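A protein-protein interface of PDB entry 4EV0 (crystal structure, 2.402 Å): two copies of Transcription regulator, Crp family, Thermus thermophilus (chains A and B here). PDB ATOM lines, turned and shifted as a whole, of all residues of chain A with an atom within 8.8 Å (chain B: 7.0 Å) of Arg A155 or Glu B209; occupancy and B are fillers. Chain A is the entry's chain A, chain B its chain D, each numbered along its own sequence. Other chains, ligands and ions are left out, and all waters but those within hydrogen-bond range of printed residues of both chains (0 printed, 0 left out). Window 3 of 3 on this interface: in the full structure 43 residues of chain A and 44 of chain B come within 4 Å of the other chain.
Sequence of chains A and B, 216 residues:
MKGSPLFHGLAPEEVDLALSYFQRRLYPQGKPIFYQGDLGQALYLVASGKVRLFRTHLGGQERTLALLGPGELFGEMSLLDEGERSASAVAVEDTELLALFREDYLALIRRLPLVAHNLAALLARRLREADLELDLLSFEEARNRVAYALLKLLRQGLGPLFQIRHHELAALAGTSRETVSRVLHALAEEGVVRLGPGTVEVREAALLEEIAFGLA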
ATOM      1  N   TYR A 148      -9.187 -30.672  20.240  1.00  0.00           N
ATOM      2  CA  TYR A 148      -8.300 -29.591  20.645  1.00  0.00           C
ATOM      3  C   TYR A 148      -6.943 -30.092  21.188  1.00  0.00           C
ATOM      4  O   TYR A 148      -5.897 -29.529  20.848  1.00  0.00           O
ATOM      5  CB  TYR A 148      -8.995 -28.737  21.688  1.00  0.00           C
ATOM      6  CG  TYR A 148      -8.367 -27.388  21.913  1.00  0.00           C
ATOM      7  CD1 TYR A 148      -8.571 -26.354  21.006  1.00  0.00           C
ATOM      8  CD2 TYR A 148      -7.597 -27.134  23.042  1.00  0.00           C
ATOM      9  CE1 TYR A 148      -8.016 -25.116  21.199  1.00  0.00           C
ATOM     10  CE2 TYR A 148      -7.034 -25.884  23.248  1.00  0.00           C
ATOM     11  CZ  TYR A 148      -7.248 -24.880  22.320  1.00  0.00           C
ATOM     12  OH  TYR A 148      -6.716 -23.627  22.495  1.00  0.00           O
ATOM     13  N   ALA A 149      -6.956 -31.135  22.024  1.00  0.00           N
ATOM     14  CA  ALA A 149      -5.696 -31.657  22.576  1.00  0.00           C
ATOM     15  C   ALA A 149      -4.765 -32.138  21.455  1.00  0.00           C
ATOM     16  O   ALA A 149      -3.594 -31.783  21.425  1.00  0.00           O
ATOM     17  CB  ALA A 149      -5.958 -32.793  23.557  1.00  0.00           C
ATOM     18  N   LEU A 150      -5.305 -32.950  20.540  1.00  0.00           N
ATOM     19  CA  LEU A 150      -4.533 -33.434  19.408  1.00  0.00           C
ATOM     20  C   LEU A 150      -4.079 -32.261  18.545  1.00  0.00           C
ATOM     21  O   LEU A 150      -2.927 -32.223  18.107  1.00  0.00           O
ATOM     22  CB  LEU A 150      -5.350 -34.397  18.555  1.00  0.00           C
ATOM     23  CG  LEU A 150      -5.680 -35.765  19.166  1.00  0.00           C
ATOM     24  CD1 LEU A 150      -6.902 -36.415  18.450  1.00  0.00           C
ATOM     25  CD2 LEU A 150      -4.449 -36.680  19.147  1.00  0.00           C
ATOM     26  N   LEU A 151      -4.986 -31.308  18.305  1.00  0.00           N
ATOM     27  CA  LEU A 151      -4.645 -30.108  17.545  1.00  0.00           C
ATOM     28  C   LEU A 151      -3.418 -29.421  18.145  1.00  0.00           C
ATOM     29  O   LEU A 151      -2.548 -28.972  17.399  1.00  0.00           O
ATOM     30  CB  LEU A 151      -5.823 -29.122  17.463  1.00  0.00           C
ATOM     31  CG  LEU A 151      -5.511 -27.811  16.716  1.00  0.00           C
ATOM     32  CD1 LEU A 151      -5.190 -28.049  15.218  1.00  0.00           C
ATOM     33  CD2 LEU A 151      -6.627 -26.758  16.873  1.00  0.00           C
ATOM     34  N   LYS A 152      -3.336 -29.350  19.477  1.00  0.00           N
ATOM     35  CA  LYS A 152      -2.182 -28.724  20.116  1.00  0.00           C
ATOM     36  C   LYS A 152      -0.875 -29.469  19.846  1.00  0.00           C
ATOM     37  O   LYS A 152       0.172 -28.847  19.691  1.00  0.00           O
ATOM     38  CB  LYS A 152      -2.384 -28.581  21.612  1.00  0.00           C
ATOM     39  CG  LYS A 152      -3.131 -27.344  22.008  1.00  0.00           C
ATOM     40  CD  LYS A 152      -3.250 -27.262  23.533  1.00  0.00           C
ATOM     41  CE  LYS A 152      -1.922 -26.872  24.159  1.00  0.00           C
ATOM     42  NZ  LYS A 152      -2.036 -26.865  25.654  1.00  0.00           N
ATOM     43  N   LEU A 153      -0.937 -30.796  19.795  1.00  0.00           N
ATOM     44  CA  LEU A 153       0.251 -31.597  19.533  1.00  0.00           C
ATOM     45  C   LEU A 153       0.738 -31.304  18.121  1.00  0.00           C
ATOM     46  O   LEU A 153       1.939 -31.177  17.873  1.00  0.00           O
ATOM     47  CB  LEU A 153      -0.043 -33.077  19.702  1.00  0.00           C
ATOM     48  CG  LEU A 153      -0.421 -33.469  21.134  1.00  0.00           C
ATOM     49  CD1 LEU A 153      -0.726 -34.953  21.213  1.00  0.00           C
ATOM     50  CD2 LEU A 153       0.690 -33.067  22.122  1.00  0.00           C
ATOM     51  N   LEU A 154      -0.216 -31.164  17.210  1.00  0.00           N
ATOM     52  CA  LEU A 154       0.060 -30.884  15.821  1.00  0.00           C
ATOM     53  C   LEU A 154       0.724 -29.507  15.672  1.00  0.00           C
ATOM     54  O   LEU A 154       1.645 -29.322  14.860  1.00  0.00           O
ATOM     55  CB  LEU A 154      -1.258 -30.907  15.074  1.00  0.00           C
ATOM     56  CG  LEU A 154      -1.298 -31.450  13.654  1.00  0.00           C
ATOM     57  CD1 LEU A 154      -0.756 -32.871  13.599  1.00  0.00           C
ATOM     58  CD2 LEU A 154      -2.760 -31.365  13.150  1.00  0.00           C
ATOM     59  N   ARG A 155       0.264 -28.552  16.475  1.00  0.00           N
ATOM     60  CA  ARG A 155       0.780 -27.197  16.421  1.00  0.00           C
ATOM     61  C   ARG A 155       2.038 -26.982  17.238  1.00  0.00           C
ATOM     62  O   ARG A 155       2.699 -25.959  17.096  1.00  0.00           O
ATOM     63  CB  ARG A 155      -0.289 -26.215  16.860  1.00  0.00           C
ATOM     64  CG  ARG A 155      -1.399 -26.120  15.852  1.00  0.00           C
ATOM     65  CD  ARG A 155      -1.901 -24.734  15.785  1.00  0.00           C
ATOM     66  NE  ARG A 155      -0.973 -23.814  15.124  1.00  0.00           N
ATOM     67  CZ  ARG A 155      -1.055 -23.460  13.839  1.00  0.00           C
ATOM     68  NH1 ARG A 155      -2.006 -23.971  13.056  1.00  0.00           N
ATOM     69  NH2 ARG A 155      -0.183 -22.597  13.324  1.00  0.00           N
ATOM     70  N   GLN A 156       2.362 -27.939  18.102  1.00  0.00           N
ATOM     71  CA  GLN A 156       3.596 -27.884  18.876  1.00  0.00           C
ATOM     72  C   GLN A 156       4.730 -28.524  18.078  1.00  0.00           C
ATOM     73  O   GLN A 156       5.864 -28.632  18.550  1.00  0.00           O
ATOM     74  CB  GLN A 156       3.411 -28.544  20.250  1.00  0.00           C
ATOM     75  CG  GLN A 156       2.737 -27.619  21.277  1.00  0.00           C
ATOM     76  CD  GLN A 156       2.251 -28.343  22.538  1.00  0.00           C
ATOM     77  OE1 GLN A 156       1.581 -29.375  22.464  1.00  0.00           O
ATOM     78  NE2 GLN A 156       2.582 -27.788  23.701  1.00  0.00           N
ATOM     79  N   GLY A 157       4.409 -28.937  16.853  1.00  0.00           N
ATOM     80  CA  GLY A 157       5.409 -29.452  15.937  1.00  0.00           C
ATOM     81  C   GLY A 157       5.314 -30.940  15.670  1.00  0.00           C
ATOM     82  O   GLY A 157       5.861 -31.434  14.685  1.00  0.00           O
ATOM     83  N   LEU A 158       4.620 -31.658  16.544  1.00  0.00           N
ATOM     84  CA  LEU A 158       4.564 -33.113  16.461  1.00  0.00           C
ATOM     85  C   LEU A 158       3.622 -33.585  15.348  1.00  0.00           C
ATOM     86  O   LEU A 158       3.002 -32.770  14.652  1.00  0.00           O
ATOM     87  CB  LEU A 158       4.147 -33.692  17.813  1.00  0.00           C
ATOM     88  CG  LEU A 158       4.922 -33.119  19.005  1.00  0.00           C
ATOM     89  CD1 LEU A 158       4.222 -33.372  20.328  1.00  0.00           C
ATOM     90  CD2 LEU A 158       6.347 -33.683  19.031  1.00  0.00           C
ATOM     91  N   GLY A 159       3.541 -34.896  15.157  1.00  0.00           N
ATOM     92  CA  GLY A 159       2.626 -35.461  14.183  1.00  0.00           C
ATOM     93  C   GLY A 159       3.016 -35.408  12.710  1.00  0.00           C
ATOM     94  O   GLY A 159       4.122 -34.991  12.353  1.00  0.00           O
ATOM     95  N   PRO A 160       2.086 -35.814  11.830  1.00  0.00           N
ATOM     96  CA  PRO A 160       0.683 -36.126  12.153  1.00  0.00           C
ATOM     97  C   PRO A 160       0.461 -37.462  12.877  1.00  0.00           C
ATOM     98  O   PRO A 160      -0.655 -37.690  13.364  1.00  0.00           O
ATOM     99  CB  PRO A 160       0.029 -36.192  10.777  1.00  0.00           C
ATOM    100  CG  PRO A 160       1.127 -36.760   9.919  1.00  0.00           C
ATOM    101  CD  PRO A 160       2.392 -36.091  10.416  1.00  0.00           C
ATOM    102  N   PHE A 162       1.009 -39.723  16.123  1.00  0.00           N
ATOM    103  CA  PHE A 162       1.417 -39.614  17.530  1.00  0.00           C
ATOM    104  C   PHE A 162       1.584 -40.962  18.213  1.00  0.00           C
ATOM    105  O   PHE A 162       0.754 -41.853  18.051  1.00  0.00           O
ATOM    106  CB  PHE A 162       0.420 -38.783  18.350  1.00  0.00           C
ATOM    107  CG  PHE A 162       0.074 -37.454  17.739  1.00  0.00           C
ATOM    108  CD1 PHE A 162       1.042 -36.462  17.593  1.00  0.00           C
ATOM    109  CD2 PHE A 162      -1.225 -37.184  17.333  1.00  0.00           C
ATOM    110  CE1 PHE A 162       0.732 -35.225  17.032  1.00  0.00           C
ATOM    111  CE2 PHE A 162      -1.550 -35.933  16.765  1.00  0.00           C
ATOM    112  CZ  PHE A 162      -0.563 -34.959  16.615  1.00  0.00           C
ATOM    113  N   VAL A 202      -3.459 -38.091  12.736  1.00  0.00           N
ATOM    114  CA  VAL A 202      -4.385 -37.108  12.188  1.00  0.00           C
ATOM    115  C   VAL A 202      -4.418 -37.222  10.665  1.00  0.00           C
ATOM    116  O   VAL A 202      -3.371 -37.139  10.013  1.00  0.00           O
ATOM    117  CB  VAL A 202      -4.029 -35.653  12.602  1.00  0.00           C
ATOM    118  CG1 VAL A 202      -4.979 -34.648  11.922  1.00  0.00           C
ATOM    119  CG2 VAL A 202      -4.079 -35.505  14.115  1.00  0.00           C
ATOM    120  N   ALA A 205      -6.376 -32.448   9.112  1.00  0.00           N
ATOM    121  CA  ALA A 205      -5.986 -31.423  10.066  1.00  0.00           C
ATOM    122  C   ALA A 205      -6.976 -30.270  10.146  1.00  0.00           C
ATOM    123  O   ALA A 205      -7.289 -29.795  11.243  1.00  0.00           O
ATOM    124  CB  ALA A 205      -4.587 -30.915   9.747  1.00  0.00           C
ATOM    125  N   LEU A 208     -10.204 -31.432  11.855  1.00  0.00           N
ATOM    126  CA  LEU A 208      -9.837 -31.554  13.261  1.00  0.00           C
ATOM    127  C   LEU A 208      -9.882 -30.203  13.966  1.00  0.00           C
ATOM    128  O   LEU A 208     -10.410 -30.083  15.078  1.00  0.00           O
ATOM    129  CB  LEU A 208      -8.432 -32.144  13.370  1.00  0.00           C
ATOM    130  CG  LEU A 208      -7.901 -32.374  14.783  1.00  0.00           C
ATOM    131  CD1 LEU A 208      -8.462 -33.663  15.437  1.00  0.00           C
ATOM    132  CD2 LEU A 208      -6.412 -32.442  14.724  1.00  0.00           C
ATOM    133  N   GLU A 209      -9.333 -29.187  13.299  1.00  0.00           N
ATOM    134  CA  GLU A 209      -9.305 -27.829  13.822  1.00  0.00           C
ATOM    135  C   GLU A 209     -10.728 -27.317  14.037  1.00  0.00           C
ATOM    136  O   GLU A 209     -11.075 -26.839  15.119  1.00  0.00           O
ATOM    137  CB  GLU A 209      -8.538 -26.906  12.860  1.00  0.00           C
ATOM    138  CG  GLU A 209      -8.228 -25.524  13.420  1.00  0.00           C
ATOM    139  CD  GLU A 209      -7.620 -24.595  12.377  1.00  0.00           C
ATOM    140  OE1 GLU A 209      -8.400 -23.918  11.678  1.00  0.00           O
ATOM    141  OE2 GLU A 209      -6.375 -24.541  12.251  1.00  0.00           O
ATOM    142  N   PHE A 213     -12.737 -26.387  17.737  1.00  0.00           N
ATOM    143  CA  PHE A 213     -13.350 -25.133  18.170  1.00  0.00           C
ATOM    144  C   PHE A 213     -14.885 -25.138  18.254  1.00  0.00           C
ATOM    145  O   PHE A 213     -15.492 -24.112  18.550  1.00  0.00           O
ATOM    146  CB  PHE A 213     -12.835 -23.946  17.347  1.00  0.00           C
ATOM    147  CG  PHE A 213     -11.388 -23.628  17.596  1.00  0.00           C
ATOM    148  CD1 PHE A 213     -11.007 -22.960  18.747  1.00  0.00           C
ATOM    149  CD2 PHE A 213     -10.407 -24.018  16.690  1.00  0.00           C
ATOM    150  CE1 PHE A 213      -9.674 -22.675  18.992  1.00  0.00           C
ATOM    151  CE2 PHE A 213      -9.065 -23.739  16.920  1.00  0.00           C
ATOM    152  CZ  PHE A 213      -8.695 -23.063  18.070  1.00  0.00           C
ATOM    153  N   ALA B 147     -10.460 -15.859  20.179  1.00  0.00           N
ATOM    154  CA  ALA B 147      -9.173 -15.576  19.560  1.00  0.00           C
ATOM    155  C   ALA B 147      -9.136 -16.210  18.173  1.00  0.00           C
ATOM    156  O   ALA B 147      -8.779 -15.556  17.202  1.00  0.00           O
ATOM    157  CB  ALA B 147      -8.032 -16.090  20.424  1.00  0.00           C
ATOM    158  N   LEU B 151      -8.539 -14.655  14.570  1.00  0.00           N
ATOM    159  CA  LEU B 151      -7.530 -15.243  13.700  1.00  0.00           C
ATOM    160  C   LEU B 151      -8.103 -15.449  12.297  1.00  0.00           C
ATOM    161  O   LEU B 151      -7.467 -15.099  11.297  1.00  0.00           O
ATOM    162  CB  LEU B 151      -7.090 -16.582  14.271  1.00  0.00           C
ATOM    163  CG  LEU B 151      -5.641 -16.989  14.122  1.00  0.00           C
ATOM    164  CD1 LEU B 151      -5.409 -18.154  15.054  1.00  0.00           C
ATOM    165  CD2 LEU B 151      -5.323 -17.378  12.681  1.00  0.00           C
ATOM    166  N   LEU B 154      -8.120 -12.277  10.440  1.00  0.00           N
ATOM    167  CA  LEU B 154      -6.753 -11.994  10.051  1.00  0.00           C
ATOM    168  C   LEU B 154      -6.366 -12.776   8.806  1.00  0.00           C
ATOM    169  O   LEU B 154      -5.586 -12.293   7.977  1.00  0.00           O
ATOM    170  CB  LEU B 154      -5.778 -12.338  11.180  1.00  0.00           C
ATOM    171  CG  LEU B 154      -5.400 -11.213  12.142  1.00  0.00           C
ATOM    172  CD1 LEU B 154      -4.404 -11.719  13.176  1.00  0.00           C
ATOM    173  CD2 LEU B 154      -4.844 -10.003  11.384  1.00  0.00           C
ATOM    174  N   ARG B 155      -6.897 -13.982   8.662  1.00  0.00           N
ATOM    175  CA  ARG B 155      -6.431 -14.819   7.572  1.00  0.00           C
ATOM    176  C   ARG B 155      -7.089 -14.542   6.210  1.00  0.00           C
ATOM    177  O   ARG B 155      -6.804 -15.218   5.219  1.00  0.00           O
ATOM    178  CB  ARG B 155      -6.391 -16.311   7.954  1.00  0.00           C
ATOM    179  CG  ARG B 155      -7.586 -16.875   8.640  1.00  0.00           C
ATOM    180  CD  ARG B 155      -7.618 -18.411   8.613  1.00  0.00           C
ATOM    181  NE  ARG B 155      -6.737 -19.074   9.568  1.00  0.00           N
ATOM    182  CZ  ARG B 155      -7.055 -20.194  10.233  1.00  0.00           C
ATOM    183  NH1 ARG B 155      -8.252 -20.758  10.061  1.00  0.00           N
ATOM    184  NH2 ARG B 155      -6.183 -20.759  11.074  1.00  0.00           N
ATOM    185  N   VAL B 192      -3.443  -7.402  23.478  1.00  0.00           N
ATOM    186  CA  VAL B 192      -3.488  -8.196  22.247  1.00  0.00           C
ATOM    187  C   VAL B 192      -4.345  -7.519  21.170  1.00  0.00           C
ATOM    188  O   VAL B 192      -4.018  -7.552  19.978  1.00  0.00           O
ATOM    189  CB  VAL B 192      -3.978  -9.645  22.520  1.00  0.00           C
ATOM    190  CG1 VAL B 192      -3.980 -10.474  21.242  1.00  0.00           C
ATOM    191  CG2 VAL B 192      -3.094 -10.301  23.579  1.00  0.00           C
ATOM    192  N   GLU B 204      -1.080  -7.772  18.460  1.00  0.00           N
ATOM    193  CA  GLU B 204      -0.151  -8.877  18.565  1.00  0.00           C
ATOM    194  C   GLU B 204      -0.719 -10.115  17.902  1.00  0.00           C
ATOM    195  O   GLU B 204      -1.273 -10.964  18.579  1.00  0.00           O
ATOM    196  CB  GLU B 204       0.073  -9.186  20.040  1.00  0.00           C
ATOM    197  CG  GLU B 204       0.378  -7.964  20.877  1.00  0.00           C
ATOM    198  CD  GLU B 204       1.775  -7.418  20.626  1.00  0.00           C
ATOM    199  OE1 GLU B 204       2.068  -6.983  19.485  1.00  0.00           O
ATOM    200  OE2 GLU B 204       2.585  -7.432  21.580  1.00  0.00           O
ATOM    201  N   ALA B 205      -0.565 -10.224  16.589  1.00  0.00           N
ATOM    202  CA  ALA B 205      -1.113 -11.354  15.845  1.00  0.00           C
ATOM    203  C   ALA B 205      -0.531 -12.697  16.269  1.00  0.00           C
ATOM    204  O   ALA B 205      -1.255 -13.690  16.358  1.00  0.00           O
ATOM    205  CB  ALA B 205      -0.935 -11.147  14.356  1.00  0.00           C
ATOM    206  N   ALA B 206       0.767 -12.736  16.537  1.00  0.00           N
ATOM    207  CA  ALA B 206       1.404 -13.986  16.908  1.00  0.00           C
ATOM    208  C   ALA B 206       0.919 -14.412  18.268  1.00  0.00           C
ATOM    209  O   ALA B 206       0.707 -15.600  18.510  1.00  0.00           O
ATOM    210  CB  ALA B 206       2.938 -13.849  16.908  1.00  0.00           C
ATOM    211  N   LEU B 207       0.764 -13.444  19.166  1.00  0.00           N
ATOM    212  CA  LEU B 207       0.326 -13.751  20.521  1.00  0.00           C
ATOM    213  C   LEU B 207      -1.131 -14.214  20.489  1.00  0.00           C
ATOM    214  O   LEU B 207      -1.546 -15.083  21.268  1.00  0.00           O
ATOM    215  CB  LEU B 207       0.488 -12.531  21.423  1.00  0.00           C
ATOM    216  CG  LEU B 207       0.152 -12.724  22.903  1.00  0.00           C
ATOM    217  CD1 LEU B 207       0.740 -14.039  23.408  1.00  0.00           C
ATOM    218  CD2 LEU B 207       0.656 -11.546  23.740  1.00  0.00           C
ATOM    219  N   LEU B 208      -1.896 -13.629  19.570  1.00  0.00           N
ATOM    220  CA  LEU B 208      -3.281 -14.015  19.368  1.00  0.00           C
ATOM    221  C   LEU B 208      -3.342 -15.470  18.910  1.00  0.00           C
ATOM    222  O   LEU B 208      -4.087 -16.271  19.472  1.00  0.00           O
ATOM    223  CB  LEU B 208      -3.943 -13.109  18.332  1.00  0.00           C
ATOM    224  CG  LEU B 208      -5.397 -13.451  18.042  1.00  0.00           C
ATOM    225  CD1 LEU B 208      -6.290 -12.955  19.185  1.00  0.00           C
ATOM    226  CD2 LEU B 208      -5.868 -12.881  16.688  1.00  0.00           C
ATOM    227  N   GLU B 209      -2.540 -15.803  17.900  1.00  0.00           N
ATOM    228  CA  GLU B 209      -2.507 -17.151  17.352  1.00  0.00           C
ATOM    229  C   GLU B 209      -2.113 -18.128  18.452  1.00  0.00           C
ATOM    230  O   GLU B 209      -2.630 -19.239  18.534  1.00  0.00           O
ATOM    231  CB  GLU B 209      -1.528 -17.227  16.178  1.00  0.00           C
ATOM    232  CG  GLU B 209      -1.697 -18.461  15.285  1.00  0.00           C
ATOM    233  CD  GLU B 209      -0.974 -18.331  13.940  1.00  0.00           C
ATOM    234  OE1 GLU B 209       0.085 -17.657  13.885  1.00  0.00           O
ATOM    235  OE2 GLU B 209      -1.472 -18.899  12.940  1.00  0.00           O
ATOM    236  N   GLU B 210      -1.214 -17.693  19.322  1.00  0.00           N
ATOM    237  CA  GLU B 210      -0.828 -18.509  20.464  1.00  0.00           C
ATOM    238  C   GLU B 210      -2.021 -18.739  21.381  1.00  0.00           C
ATOM    239  O   GLU B 210      -2.247 -19.849  21.850  1.00  0.00           O
ATOM    240  CB  GLU B 210       0.324 -17.864  21.249  1.00  0.00           C
ATOM    241  CG  GLU B 210       1.674 -17.878  20.538  1.00  0.00           C
ATOM    242  CD  GLU B 210       2.843 -17.617  21.490  1.00  0.00           C
ATOM    243  OE1 GLU B 210       2.615 -17.060  22.590  1.00  0.00           O
ATOM    244  OE2 GLU B 210       3.992 -17.976  21.143  1.00  0.00           O
ATOM    245  N   ILE B 211      -2.776 -17.677  21.638  1.00  0.00           N
ATOM    246  CA  ILE B 211      -3.942 -17.768  22.511  1.00  0.00           C
ATOM    247  C   ILE B 211      -5.034 -18.655  21.901  1.00  0.00           C
ATOM    248  O   ILE B 211      -5.670 -19.426  22.622  1.00  0.00           O
ATOM    249  CB  ILE B 211      -4.508 -16.364  22.883  1.00  0.00           C
ATOM    250  CG1 ILE B 211      -3.488 -15.592  23.726  1.00  0.00           C
ATOM    251  CG2 ILE B 211      -5.811 -16.499  23.670  1.00  0.00           C
ATOM    252  CD1 ILE B 211      -3.839 -14.136  23.946  1.00  0.00           C
ATOM    253  N   ALA B 212      -5.230 -18.558  20.580  1.00  0.00           N
ATOM    254  CA  ALA B 212      -6.247 -19.360  19.893  1.00  0.00           C
ATOM    255  C   ALA B 212      -5.979 -20.855  20.072  1.00  0.00           C
ATOM    256  O   ALA B 212      -6.898 -21.652  20.283  1.00  0.00           O
ATOM    257  CB  ALA B 212      -6.321 -19.011  18.420  1.00  0.00           C
ATOM    258  N   PHE B 213      -4.707 -21.228  20.006  1.00  0.00           N
ATOM    259  CA  PHE B 213      -4.341 -22.631  20.087  1.00  0.00           C
ATOM    260  C   PHE B 213      -3.937 -23.044  21.478  1.00  0.00           C
ATOM    261  O   PHE B 213      -3.385 -24.123  21.674  1.00  0.00           O
ATOM    262  CB  PHE B 213      -3.272 -22.966  19.059  1.00  0.00           C
ATOM    263  CG  PHE B 213      -3.752 -22.788  17.669  1.00  0.00           C
ATOM    264  CD1 PHE B 213      -4.754 -23.615  17.166  1.00  0.00           C
ATOM    265  CD2 PHE B 213      -3.273 -21.762  16.876  1.00  0.00           C
ATOM    266  CE1 PHE B 213      -5.229 -23.456  15.872  1.00  0.00           C
ATOM    267  CE2 PHE B 213      -3.746 -21.592  15.581  1.00  0.00           C
ATOM    268  CZ  PHE B 213      -4.728 -22.441  15.079  1.00  0.00           C
ATOM    269  N   GLY B 214      -4.254 -22.203  22.454  1.00  0.00           N
ATOM    270  CA  GLY B 214      -4.207 -22.615  23.849  1.00  0.00           C
ATOM    271  C   GLY B 214      -2.822 -22.872  24.418  1.00  0.00           C
ATOM    272  O   GLY B 214      -2.662 -23.493  25.480  1.00  0.00           O
ATOM    273  N   LEU B 215      -1.803 -22.399  23.716  1.00  0.00           N
ATOM    274  CA  LEU B 215      -0.467 -22.431  24.281  1.00  0.00           C
ATOM    275  C   LEU B 215      -0.104 -21.075  24.898  1.00  0.00           C
ATOM    276  O   LEU B 215       1.017 -20.865  25.347  1.00  0.00           O
ATOM    277  CB  LEU B 215       0.570 -22.929  23.261  1.00  0.00           C
ATOM    278  CG  LEU B 215       0.363 -22.662  21.766  1.00  0.00           C
ATOM    279  CD1 LEU B 215       1.091 -21.406  21.355  1.00  0.00           C
ATOM    280  CD2 LEU B 215       0.821 -23.849  20.917  1.00  0.00           C
ATOM    281  N   ALA B 216      -1.074 -20.166  24.931  1.00  0.00           N
ATOM    282  CA  ALA B 216      -0.952 -18.912  25.669  1.00  0.00           C
ATOM    283  C   ALA B 216      -2.344 -18.452  26.105  1.00  0.00           C
ATOM    284  O   ALA B 216      -2.530 -17.387  26.672  1.00  0.00           O
ATOM    285  CB  ALA B 216      -0.264 -17.852  24.828  1.00  0.00           C
ATOM    286  OXT ALA B 216      -3.343 -19.145  25.902  1.00  0.00           O
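The side-chain hydroxyl of Tyr A148 lies within hydrogen-bond range of the backbone carbonyl oxygen of Ala B212. OH of Tyr A148 lies close to O of Phe B213, 3.5 Å away. OH of Tyr A148 sits at hydrogen-bond distance from N of Gly B214, 2.8 Å away. The backbone carbonyl oxygen (O) of Gly B214 lies within hydrogen-bond range of the side-chain amino group (NZ) of Lys A152 (3.4 Å). OE2 of Glu B209 lies within salt-bridge range of NH2 of Arg A155 (3.9 Å). The side-chain carboxylate (OE1) of Glu A209 is in salt-bridge range of the guanidinium group (NH1) of Arg B155 (3.6 Å).
The backbone carbonyl oxygen of Lys A152 sits close to the side-chain amide oxygen of Gln A156.
Leu A151 touches Phe B213, but with the chains exchanged Phe A213 does not touch Leu B151 (6.6 Å). Arg A155 touches Glu B209, and with the chains exchanged Glu A209 touches Arg B155. Arg A155 touches Phe B213, but with the chains exchanged Phe A213 does not touch Arg B155 (7.2 Å). Glu A209 touches Phe B213, but with the chains exchanged Phe A213 does not touch Glu B209 (7.2 Å). Of the 12 pairs that touch across the chains among the printed residues, 3 have their exchanged pair printed and touching as well.
Of the printed residues of chain B, Leu A151 touches Phe B213 (3.7 Å). Arg A155 touches two residues of chain B. Of the printed residues of chain B, Glu A209 touches Arg B155 (3.6 Å) and Phe B213 (3.9 Å). Glu B210 touches none of the printed residues of chain A. Of the printed residues of chain A, Ala B212 touches Tyr A148 and Phe A213. The nearest residue of chain B that does not touch Arg A155 is Leu B215 (4.8 Å). The nearest printed residue of chain A that does not touch Glu B209 is Phe A213 (7.2 Å).
Among the printed residues, pairs that only touch across the chains: Leu A151 with Phe B213, Lys A152 with Phe B213, Arg A155 with Phe B213, Glu A209 with Phe B213, Phe A213 with Ala B212 and Phe A213 with Phe B213.
Of the 18 printed residues of chain B, 5 touch a printed residue of chain A. Printed residues of chain B that touch a printed residue of chain A: Arg B155, Glu B209, Ala B212, Phe B213 and Gly B214. Among the printed residues, Asp or Glu carboxylates within 4 Å of a Lys or Arg side-chain nitrogen of the other chain: Arg A155 with Glu B209 (3.9 Å) and Glu A209 with Arg B155 (3.6 Å).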
